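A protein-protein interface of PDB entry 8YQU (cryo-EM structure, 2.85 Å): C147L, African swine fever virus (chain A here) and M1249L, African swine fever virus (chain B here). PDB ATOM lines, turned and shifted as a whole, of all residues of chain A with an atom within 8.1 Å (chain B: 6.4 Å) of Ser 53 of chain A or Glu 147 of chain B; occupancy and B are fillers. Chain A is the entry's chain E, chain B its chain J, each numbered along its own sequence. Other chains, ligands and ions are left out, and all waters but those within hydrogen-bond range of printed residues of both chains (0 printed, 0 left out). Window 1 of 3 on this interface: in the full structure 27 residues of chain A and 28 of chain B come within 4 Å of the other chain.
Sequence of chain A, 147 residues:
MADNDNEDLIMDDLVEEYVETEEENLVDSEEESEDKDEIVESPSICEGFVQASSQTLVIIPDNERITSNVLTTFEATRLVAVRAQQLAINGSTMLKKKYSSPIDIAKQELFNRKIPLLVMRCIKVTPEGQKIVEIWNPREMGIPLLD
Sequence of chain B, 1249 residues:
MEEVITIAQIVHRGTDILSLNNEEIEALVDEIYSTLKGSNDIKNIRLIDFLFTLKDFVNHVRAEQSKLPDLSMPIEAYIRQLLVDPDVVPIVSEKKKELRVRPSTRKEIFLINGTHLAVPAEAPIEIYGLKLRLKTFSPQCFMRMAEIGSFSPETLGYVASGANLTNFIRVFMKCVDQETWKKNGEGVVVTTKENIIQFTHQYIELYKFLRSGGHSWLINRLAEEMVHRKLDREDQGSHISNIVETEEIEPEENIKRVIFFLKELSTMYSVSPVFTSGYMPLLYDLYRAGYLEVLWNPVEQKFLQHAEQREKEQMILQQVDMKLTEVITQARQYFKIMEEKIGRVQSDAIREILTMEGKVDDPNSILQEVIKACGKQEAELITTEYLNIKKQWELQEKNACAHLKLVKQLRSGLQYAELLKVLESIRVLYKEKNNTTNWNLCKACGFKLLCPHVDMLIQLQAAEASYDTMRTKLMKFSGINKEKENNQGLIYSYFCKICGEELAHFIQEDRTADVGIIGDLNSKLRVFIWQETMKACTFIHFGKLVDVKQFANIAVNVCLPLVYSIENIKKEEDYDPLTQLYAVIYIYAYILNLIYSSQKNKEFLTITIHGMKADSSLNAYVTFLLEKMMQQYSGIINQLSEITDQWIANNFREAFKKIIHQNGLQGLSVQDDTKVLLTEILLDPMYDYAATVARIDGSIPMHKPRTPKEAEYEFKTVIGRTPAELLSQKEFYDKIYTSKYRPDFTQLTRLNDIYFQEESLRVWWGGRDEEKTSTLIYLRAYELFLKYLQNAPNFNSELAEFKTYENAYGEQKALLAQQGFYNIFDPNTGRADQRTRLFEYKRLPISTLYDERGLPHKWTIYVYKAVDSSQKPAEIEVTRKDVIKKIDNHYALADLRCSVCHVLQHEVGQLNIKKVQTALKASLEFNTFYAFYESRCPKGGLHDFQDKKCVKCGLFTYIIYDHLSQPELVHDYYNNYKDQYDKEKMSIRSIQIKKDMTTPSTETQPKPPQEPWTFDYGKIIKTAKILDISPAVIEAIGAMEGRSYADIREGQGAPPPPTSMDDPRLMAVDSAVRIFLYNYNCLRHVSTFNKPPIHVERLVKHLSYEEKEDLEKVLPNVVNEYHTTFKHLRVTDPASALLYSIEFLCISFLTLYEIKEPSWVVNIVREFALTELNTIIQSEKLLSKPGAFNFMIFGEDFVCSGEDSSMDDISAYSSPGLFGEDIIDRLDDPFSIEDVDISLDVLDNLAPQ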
ATOM      1  N   PHE A  49      21.580  -1.279  -4.471  1.00  0.00           N
ATOM      2  CA  PHE A  49      21.404  -2.669  -4.866  1.00  0.00           C
ATOM      3  C   PHE A  49      21.940  -3.593  -3.783  1.00  0.00           C
ATOM      4  O   PHE A  49      23.035  -3.377  -3.254  1.00  0.00           O
ATOM      5  CB  PHE A  49      22.117  -2.951  -6.188  1.00  0.00           C
ATOM      6  CG  PHE A  49      21.423  -2.378  -7.389  1.00  0.00           C
ATOM      7  CD1 PHE A  49      20.162  -2.818  -7.750  1.00  0.00           C
ATOM      8  CD2 PHE A  49      22.038  -1.410  -8.164  1.00  0.00           C
ATOM      9  CE1 PHE A  49      19.523  -2.297  -8.857  1.00  0.00           C
ATOM     10  CE2 PHE A  49      21.404  -0.886  -9.271  1.00  0.00           C
ATOM     11  CZ  PHE A  49      20.145  -1.329  -9.617  1.00  0.00           C
ATOM     12  N   VAL A  50      21.165  -4.624  -3.453  1.00  0.00           N
ATOM     13  CA  VAL A  50      21.613  -5.643  -2.511  1.00  0.00           C
ATOM     14  C   VAL A  50      22.188  -6.866  -3.221  1.00  0.00           C
ATOM     15  O   VAL A  50      23.195  -7.421  -2.753  1.00  0.00           O
ATOM     16  CB  VAL A  50      20.467  -6.059  -1.566  1.00  0.00           C
ATOM     17  CG1 VAL A  50      20.909  -7.184  -0.643  1.00  0.00           C
ATOM     18  CG2 VAL A  50      19.984  -4.863  -0.762  1.00  0.00           C
ATOM     19  N   GLN A  51      21.602  -7.283  -4.340  1.00  0.00           N
ATOM     20  CA  GLN A  51      22.076  -8.449  -5.078  1.00  0.00           C
ATOM     21  C   GLN A  51      23.418  -8.124  -5.722  1.00  0.00           C
ATOM     22  O   GLN A  51      23.520  -7.195  -6.530  1.00  0.00           O
ATOM     23  CB  GLN A  51      21.054  -8.865  -6.130  1.00  0.00           C
ATOM     24  CG  GLN A  51      21.439 -10.114  -6.902  1.00  0.00           C
ATOM     25  CD  GLN A  51      20.452 -10.445  -8.000  1.00  0.00           C
ATOM     26  OE1 GLN A  51      19.259 -10.167  -7.884  1.00  0.00           O
ATOM     27  NE2 GLN A  51      20.947 -11.040  -9.079  1.00  0.00           N
ATOM     28  N   ALA A  52      24.447  -8.886  -5.364  1.00  0.00           N
ATOM     29  CA  ALA A  52      25.757  -8.710  -5.974  1.00  0.00           C
ATOM     30  C   ALA A  52      25.734  -9.168  -7.426  1.00  0.00           C
ATOM     31  O   ALA A  52      25.009 -10.098  -7.791  1.00  0.00           O
ATOM     32  CB  ALA A  52      26.816  -9.486  -5.194  1.00  0.00           C
ATOM     33  N   SER A  53      26.531  -8.503  -8.258  1.00  0.00           N
ATOM     34  CA  SER A  53      26.587  -8.840  -9.671  1.00  0.00           C
ATOM     35  C   SER A  53      27.192 -10.225  -9.873  1.00  0.00           C
ATOM     36  O   SER A  53      28.027 -10.685  -9.090  1.00  0.00           O
ATOM     37  CB  SER A  53      27.402  -7.797 -10.436  1.00  0.00           C
ATOM     38  OG  SER A  53      26.777  -6.526 -10.382  1.00  0.00           O
ATOM     39  N   SER A  54      26.759 -10.890 -10.941  1.00  0.00           N
ATOM     40  CA  SER A  54      27.244 -12.228 -11.239  1.00  0.00           C
ATOM     41  C   SER A  54      28.713 -12.187 -11.650  1.00  0.00           C
ATOM     42  O   SER A  54      29.250 -11.149 -12.046  1.00  0.00           O
ATOM     43  CB  SER A  54      26.406 -12.870 -12.342  1.00  0.00           C
ATOM     44  OG  SER A  54      25.057 -13.015 -11.935  1.00  0.00           O
ATOM     45  N   GLN A  55      29.362 -13.342 -11.553  1.00  0.00           N
ATOM     46  CA  GLN A  55      30.792 -13.455 -11.777  1.00  0.00           C
ATOM     47  C   GLN A  55      31.076 -14.390 -12.945  1.00  0.00           C
ATOM     48  O   GLN A  55      30.258 -15.242 -13.303  1.00  0.00           O
ATOM     49  CB  GLN A  55      31.505 -13.961 -10.518  1.00  0.00           C
ATOM     50  CG  GLN A  55      31.460 -12.988  -9.356  1.00  0.00           C
ATOM     51  CD  GLN A  55      31.916 -13.614  -8.056  1.00  0.00           C
ATOM     52  OE1 GLN A  55      32.146 -14.820  -7.982  1.00  0.00           O
ATOM     53  NE2 GLN A  55      32.045 -12.796  -7.020  1.00  0.00           N
ATOM     54  N   THR A  56      32.251 -14.215 -13.540  1.00  0.00           N
ATOM     55  CA  THR A  56      32.730 -15.062 -14.623  1.00  0.00           C
ATOM     56  C   THR A  56      33.907 -15.886 -14.123  1.00  0.00           C
ATOM     57  O   THR A  56      34.886 -15.331 -13.617  1.00  0.00           O
ATOM     58  CB  THR A  56      33.150 -14.229 -15.836  1.00  0.00           C
ATOM     59  OG1 THR A  56      32.146 -13.248 -16.117  1.00  0.00           O
ATOM     60  CG2 THR A  56      33.335 -15.121 -17.051  1.00  0.00           C
ATOM     61  N   VAL A 125      38.887 -13.108  -6.168  1.00  0.00           N
ATOM     62  CA  VAL A 125      37.682 -12.500  -6.717  1.00  0.00           C
ATOM     63  C   VAL A 125      37.984 -11.035  -7.002  1.00  0.00           C
ATOM     64  O   VAL A 125      38.151 -10.233  -6.075  1.00  0.00           O
ATOM     65  CB  VAL A 125      36.490 -12.642  -5.758  1.00  0.00           C
ATOM     66  CG1 VAL A 125      35.275 -11.930  -6.321  1.00  0.00           C
ATOM     67  CG2 VAL A 125      36.188 -14.110  -5.510  1.00  0.00           C
ATOM     68  N   PRO A 127      37.448  -7.157  -8.482  1.00  0.00           N
ATOM     69  CA  PRO A 127      36.331  -6.200  -8.418  1.00  0.00           C
ATOM     70  C   PRO A 127      35.535  -6.081  -9.707  1.00  0.00           C
ATOM     71  O   PRO A 127      34.323  -5.839  -9.647  1.00  0.00           O
ATOM     72  CB  PRO A 127      37.031  -4.881  -8.068  1.00  0.00           C
ATOM     73  CG  PRO A 127      38.224  -5.301  -7.294  1.00  0.00           C
ATOM     74  CD  PRO A 127      38.686  -6.590  -7.919  1.00  0.00           C
ATOM     75  N   GLU A 128      36.168  -6.237 -10.872  1.00  0.00           N
ATOM     76  CA  GLU A 128      35.427  -6.100 -12.121  1.00  0.00           C
ATOM     77  C   GLU A 128      34.456  -7.248 -12.361  1.00  0.00           C
ATOM     78  O   GLU A 128      33.587  -7.126 -13.231  1.00  0.00           O
ATOM     79  CB  GLU A 128      36.385  -5.986 -13.309  1.00  0.00           C
ATOM     80  CG  GLU A 128      37.199  -7.234 -13.585  1.00  0.00           C
ATOM     81  CD  GLU A 128      38.171  -7.052 -14.733  1.00  0.00           C
ATOM     82  OE1 GLU A 128      38.225  -5.939 -15.298  1.00  0.00           O
ATOM     83  OE2 GLU A 128      38.881  -8.020 -15.072  1.00  0.00           O
ATOM     84  N   GLY A 129      34.578  -8.349 -11.623  1.00  0.00           N
ATOM     85  CA  GLY A 129      33.622  -9.431 -11.736  1.00  0.00           C
ATOM     86  C   GLY A 129      34.231 -10.807 -11.906  1.00  0.00           C
ATOM     87  O   GLY A 129      33.575 -11.812 -11.624  1.00  0.00           O
ATOM     88  N   PHE B 142      22.240  -0.138 -15.692  1.00  0.00           N
ATOM     89  CA  PHE B 142      21.231  -0.804 -16.506  1.00  0.00           C
ATOM     90  C   PHE B 142      21.612  -2.255 -16.765  1.00  0.00           C
ATOM     91  O   PHE B 142      20.752  -3.144 -16.744  1.00  0.00           O
ATOM     92  CB  PHE B 142      21.034  -0.047 -17.817  1.00  0.00           C
ATOM     93  CG  PHE B 142      19.897  -0.559 -18.648  1.00  0.00           C
ATOM     94  CD1 PHE B 142      18.589  -0.375 -18.236  1.00  0.00           C
ATOM     95  CD2 PHE B 142      20.132  -1.218 -19.841  1.00  0.00           C
ATOM     96  CE1 PHE B 142      17.537  -0.843 -18.997  1.00  0.00           C
ATOM     97  CE2 PHE B 142      19.085  -1.688 -20.605  1.00  0.00           C
ATOM     98  CZ  PHE B 142      17.787  -1.500 -20.183  1.00  0.00           C
ATOM     99  N   MET B 143      22.901  -2.516 -16.999  1.00  0.00           N
ATOM    100  CA  MET B 143      23.363  -3.892 -17.155  1.00  0.00           C
ATOM    101  C   MET B 143      23.150  -4.698 -15.881  1.00  0.00           C
ATOM    102  O   MET B 143      22.787  -5.876 -15.940  1.00  0.00           O
ATOM    103  CB  MET B 143      24.834  -3.912 -17.566  1.00  0.00           C
ATOM    104  CG  MET B 143      25.092  -3.359 -18.956  1.00  0.00           C
ATOM    105  SD  MET B 143      24.268  -4.342 -20.227  1.00  0.00           S
ATOM    106  CE  MET B 143      22.844  -3.321 -20.592  1.00  0.00           C
ATOM    107  N   ARG B 144      23.374  -4.083 -14.720  1.00  0.00           N
ATOM    108  CA  ARG B 144      23.157  -4.785 -13.460  1.00  0.00           C
ATOM    109  C   ARG B 144      21.682  -5.116 -13.256  1.00  0.00           C
ATOM    110  O   ARG B 144      21.345  -6.219 -12.806  1.00  0.00           O
ATOM    111  CB  ARG B 144      23.692  -3.950 -12.299  1.00  0.00           C
ATOM    112  CG  ARG B 144      23.788  -4.699 -10.984  1.00  0.00           C
ATOM    113  CD  ARG B 144      24.424  -3.831  -9.914  1.00  0.00           C
ATOM    114  NE  ARG B 144      24.594  -4.544  -8.655  1.00  0.00           N
ATOM    115  CZ  ARG B 144      25.097  -4.006  -7.554  1.00  0.00           C
ATOM    116  NH1 ARG B 144      25.494  -2.744  -7.521  1.00  0.00           N
ATOM    117  NH2 ARG B 144      25.202  -4.750  -6.457  1.00  0.00           N
ATOM    118  N   MET B 145      20.787  -4.178 -13.579  1.00  0.00           N
ATOM    119  CA  MET B 145      19.360  -4.475 -13.458  1.00  0.00           C
ATOM    120  C   MET B 145      18.937  -5.564 -14.436  1.00  0.00           C
ATOM    121  O   MET B 145      18.130  -6.436 -14.094  1.00  0.00           O
ATOM    122  CB  MET B 145      18.515  -3.226 -13.682  1.00  0.00           C
ATOM    123  CG  MET B 145      18.672  -2.157 -12.634  1.00  0.00           C
ATOM    124  SD  MET B 145      17.520  -0.831 -13.000  1.00  0.00           S
ATOM    125  CE  MET B 145      18.321  -0.158 -14.441  1.00  0.00           C
ATOM    126  N   ALA B 146      19.454  -5.518 -15.666  1.00  0.00           N
ATOM    127  CA  ALA B 146      19.144  -6.566 -16.631  1.00  0.00           C
ATOM    128  C   ALA B 146      19.692  -7.915 -16.180  1.00  0.00           C
ATOM    129  O   ALA B 146      19.083  -8.955 -16.453  1.00  0.00           O
ATOM    130  CB  ALA B 146      19.694  -6.192 -18.004  1.00  0.00           C
ATOM    131  N   GLU B 147      20.840  -7.914 -15.498  1.00  0.00           N
ATOM    132  CA  GLU B 147      21.341  -9.131 -14.872  1.00  0.00           C
ATOM    133  C   GLU B 147      20.372  -9.628 -13.809  1.00  0.00           C
ATOM    134  O   GLU B 147      20.110 -10.832 -13.710  1.00  0.00           O
ATOM    135  CB  GLU B 147      22.722  -8.891 -14.259  1.00  0.00           C
ATOM    136  CG  GLU B 147      23.818  -8.625 -15.279  1.00  0.00           C
ATOM    137  CD  GLU B 147      25.154  -8.321 -14.630  1.00  0.00           C
ATOM    138  OE1 GLU B 147      25.188  -8.131 -13.397  1.00  0.00           O
ATOM    139  OE2 GLU B 147      26.171  -8.270 -15.355  1.00  0.00           O
ATOM    140  N   ILE B 148      19.835  -8.714 -12.999  1.00  0.00           N
ATOM    141  CA  ILE B 148      18.735  -9.076 -12.109  1.00  0.00           C
ATOM    142  C   ILE B 148      17.520  -9.496 -12.927  1.00  0.00           C
ATOM    143  O   ILE B 148      16.883 -10.518 -12.643  1.00  0.00           O
ATOM    144  CB  ILE B 148      18.405  -7.909 -11.160  1.00  0.00           C
ATOM    145  CG1 ILE B 148      19.602  -7.595 -10.260  1.00  0.00           C
ATOM    146  CG2 ILE B 148      17.179  -8.230 -10.324  1.00  0.00           C
ATOM    147  CD1 ILE B 148      19.402  -6.374  -9.388  1.00  0.00           C
ATOM    148  N   GLY B 149      17.185  -8.718 -13.953  1.00  0.00           N
ATOM    149  CA  GLY B 149      16.172  -9.108 -14.917  1.00  0.00           C
ATOM    150  C   GLY B 149      14.782  -9.310 -14.360  1.00  0.00           C
ATOM    151  O   GLY B 149      14.050 -10.178 -14.846  1.00  0.00           O
ATOM    152  N   SER B 150      14.391  -8.530 -13.352  1.00  0.00           N
ATOM    153  CA  SER B 150      13.053  -8.642 -12.786  1.00  0.00           C
ATOM    154  C   SER B 150      12.466  -7.274 -12.463  1.00  0.00           C
ATOM    155  O   SER B 150      11.673  -7.142 -11.525  1.00  0.00           O
ATOM    156  CB  SER B 150      13.058  -9.516 -11.534  1.00  0.00           C
ATOM    157  OG  SER B 150      14.039  -9.078 -10.612  1.00  0.00           O
ATOM    158  N   VAL B 227      22.309  -7.804 -23.014  1.00  0.00           N
ATOM    159  CA  VAL B 227      22.785  -8.926 -22.206  1.00  0.00           C
ATOM    160  C   VAL B 227      23.341 -10.027 -23.099  1.00  0.00           C
ATOM    161  O   VAL B 227      24.402 -10.599 -22.817  1.00  0.00           O
ATOM    162  CB  VAL B 227      21.661  -9.451 -21.293  1.00  0.00           C
ATOM    163  CG1 VAL B 227      22.095 -10.732 -20.604  1.00  0.00           C
ATOM    164  CG2 VAL B 227      21.297  -8.408 -20.263  1.00  0.00           C
ATOM    165  N   LYS B 230      26.696  -8.983 -24.404  1.00  0.00           N
ATOM    166  CA  LYS B 230      27.711  -9.151 -23.367  1.00  0.00           C
ATOM    167  C   LYS B 230      28.121 -10.615 -23.232  1.00  0.00           C
ATOM    168  O   LYS B 230      29.314 -10.939 -23.117  1.00  0.00           O
ATOM    169  CB  LYS B 230      27.184  -8.612 -22.037  1.00  0.00           C
ATOM    170  CG  LYS B 230      28.201  -8.593 -20.908  1.00  0.00           C
ATOM    171  CD  LYS B 230      27.600  -7.977 -19.654  1.00  0.00           C
ATOM    172  CE  LYS B 230      28.647  -7.775 -18.571  1.00  0.00           C
ATOM    173  NZ  LYS B 230      28.077  -7.098 -17.373  1.00  0.00           N
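Among the printed residues, pairs that only touch across the chains: Phe 49 of chain A with Arg 144 of chain B (3.4 Å), Phe 49 of chain A with Met 145 of chain B (3.5 Å), Phe 49 of chain A with Ile 148 of chain B (3.99 Å), Gln 51 of chain A with Ile 148 of chain B (3.5 Å) and Ser 53 of chain A with Glu 147 of chain B (3.7 Å).
Of the printed residues of chain B, Ser 53 of chain A touches Arg 144 (3.4 Å) and Glu 147 (3.7 Å).
Thr 56 of chain A touches none of the printed residues of chain B.
Met 143 of chain B touches none of the printed residues of chain A.
Printed residues of chain A within 4 Å of Arg 144 of chain B: Phe 49, Gln 51 and Ser 53.
Of the printed residues of chain A, Met 145 of chain B touches Phe 49.
Ala 146 of chain B touches none of the printed residues of chain A.
Printed residues of chain A within 4 Å of Ile 148 of chain B: Phe 49 and Gln 51.
The nearest printed residue of chain A that does not touch Arg 144 of chain B is Ala 52 of chain A (4.03 Å).
O of Gln 51 of chain A is in hydrogen-bond range of NH2 of Arg 144 of chain B (3.0 Å).
The side-chain hydroxyl of Ser 53 of chain A sits at hydrogen-bond distance from the guanidinium group of Arg 144 of chain B (3.4 Å).
Of the 12 printed residues of chain A, 3 touch a printed residue of chain B.
Hydrophobic or aromatic side chains of chain A within 4 Å of the printed part of chain B: Phe 49.
Hydrophobic or aromatic side chains of chain B within 4 Å of the printed part of chain A: Met 145 and Ile 148.
Among the printed residues, 7 pairs touch across the chains.
Among the printed residues, no Asp or Glu carboxylate lies within 4 Å of a Lys or Arg side-chain nitrogen of the other chain.
The side-chain amino group (NZ) of Lys 230 of chain B is in salt-bridge range of the side-chain carboxylate (OE2) of Glu 147 of chain B (3.0 Å).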
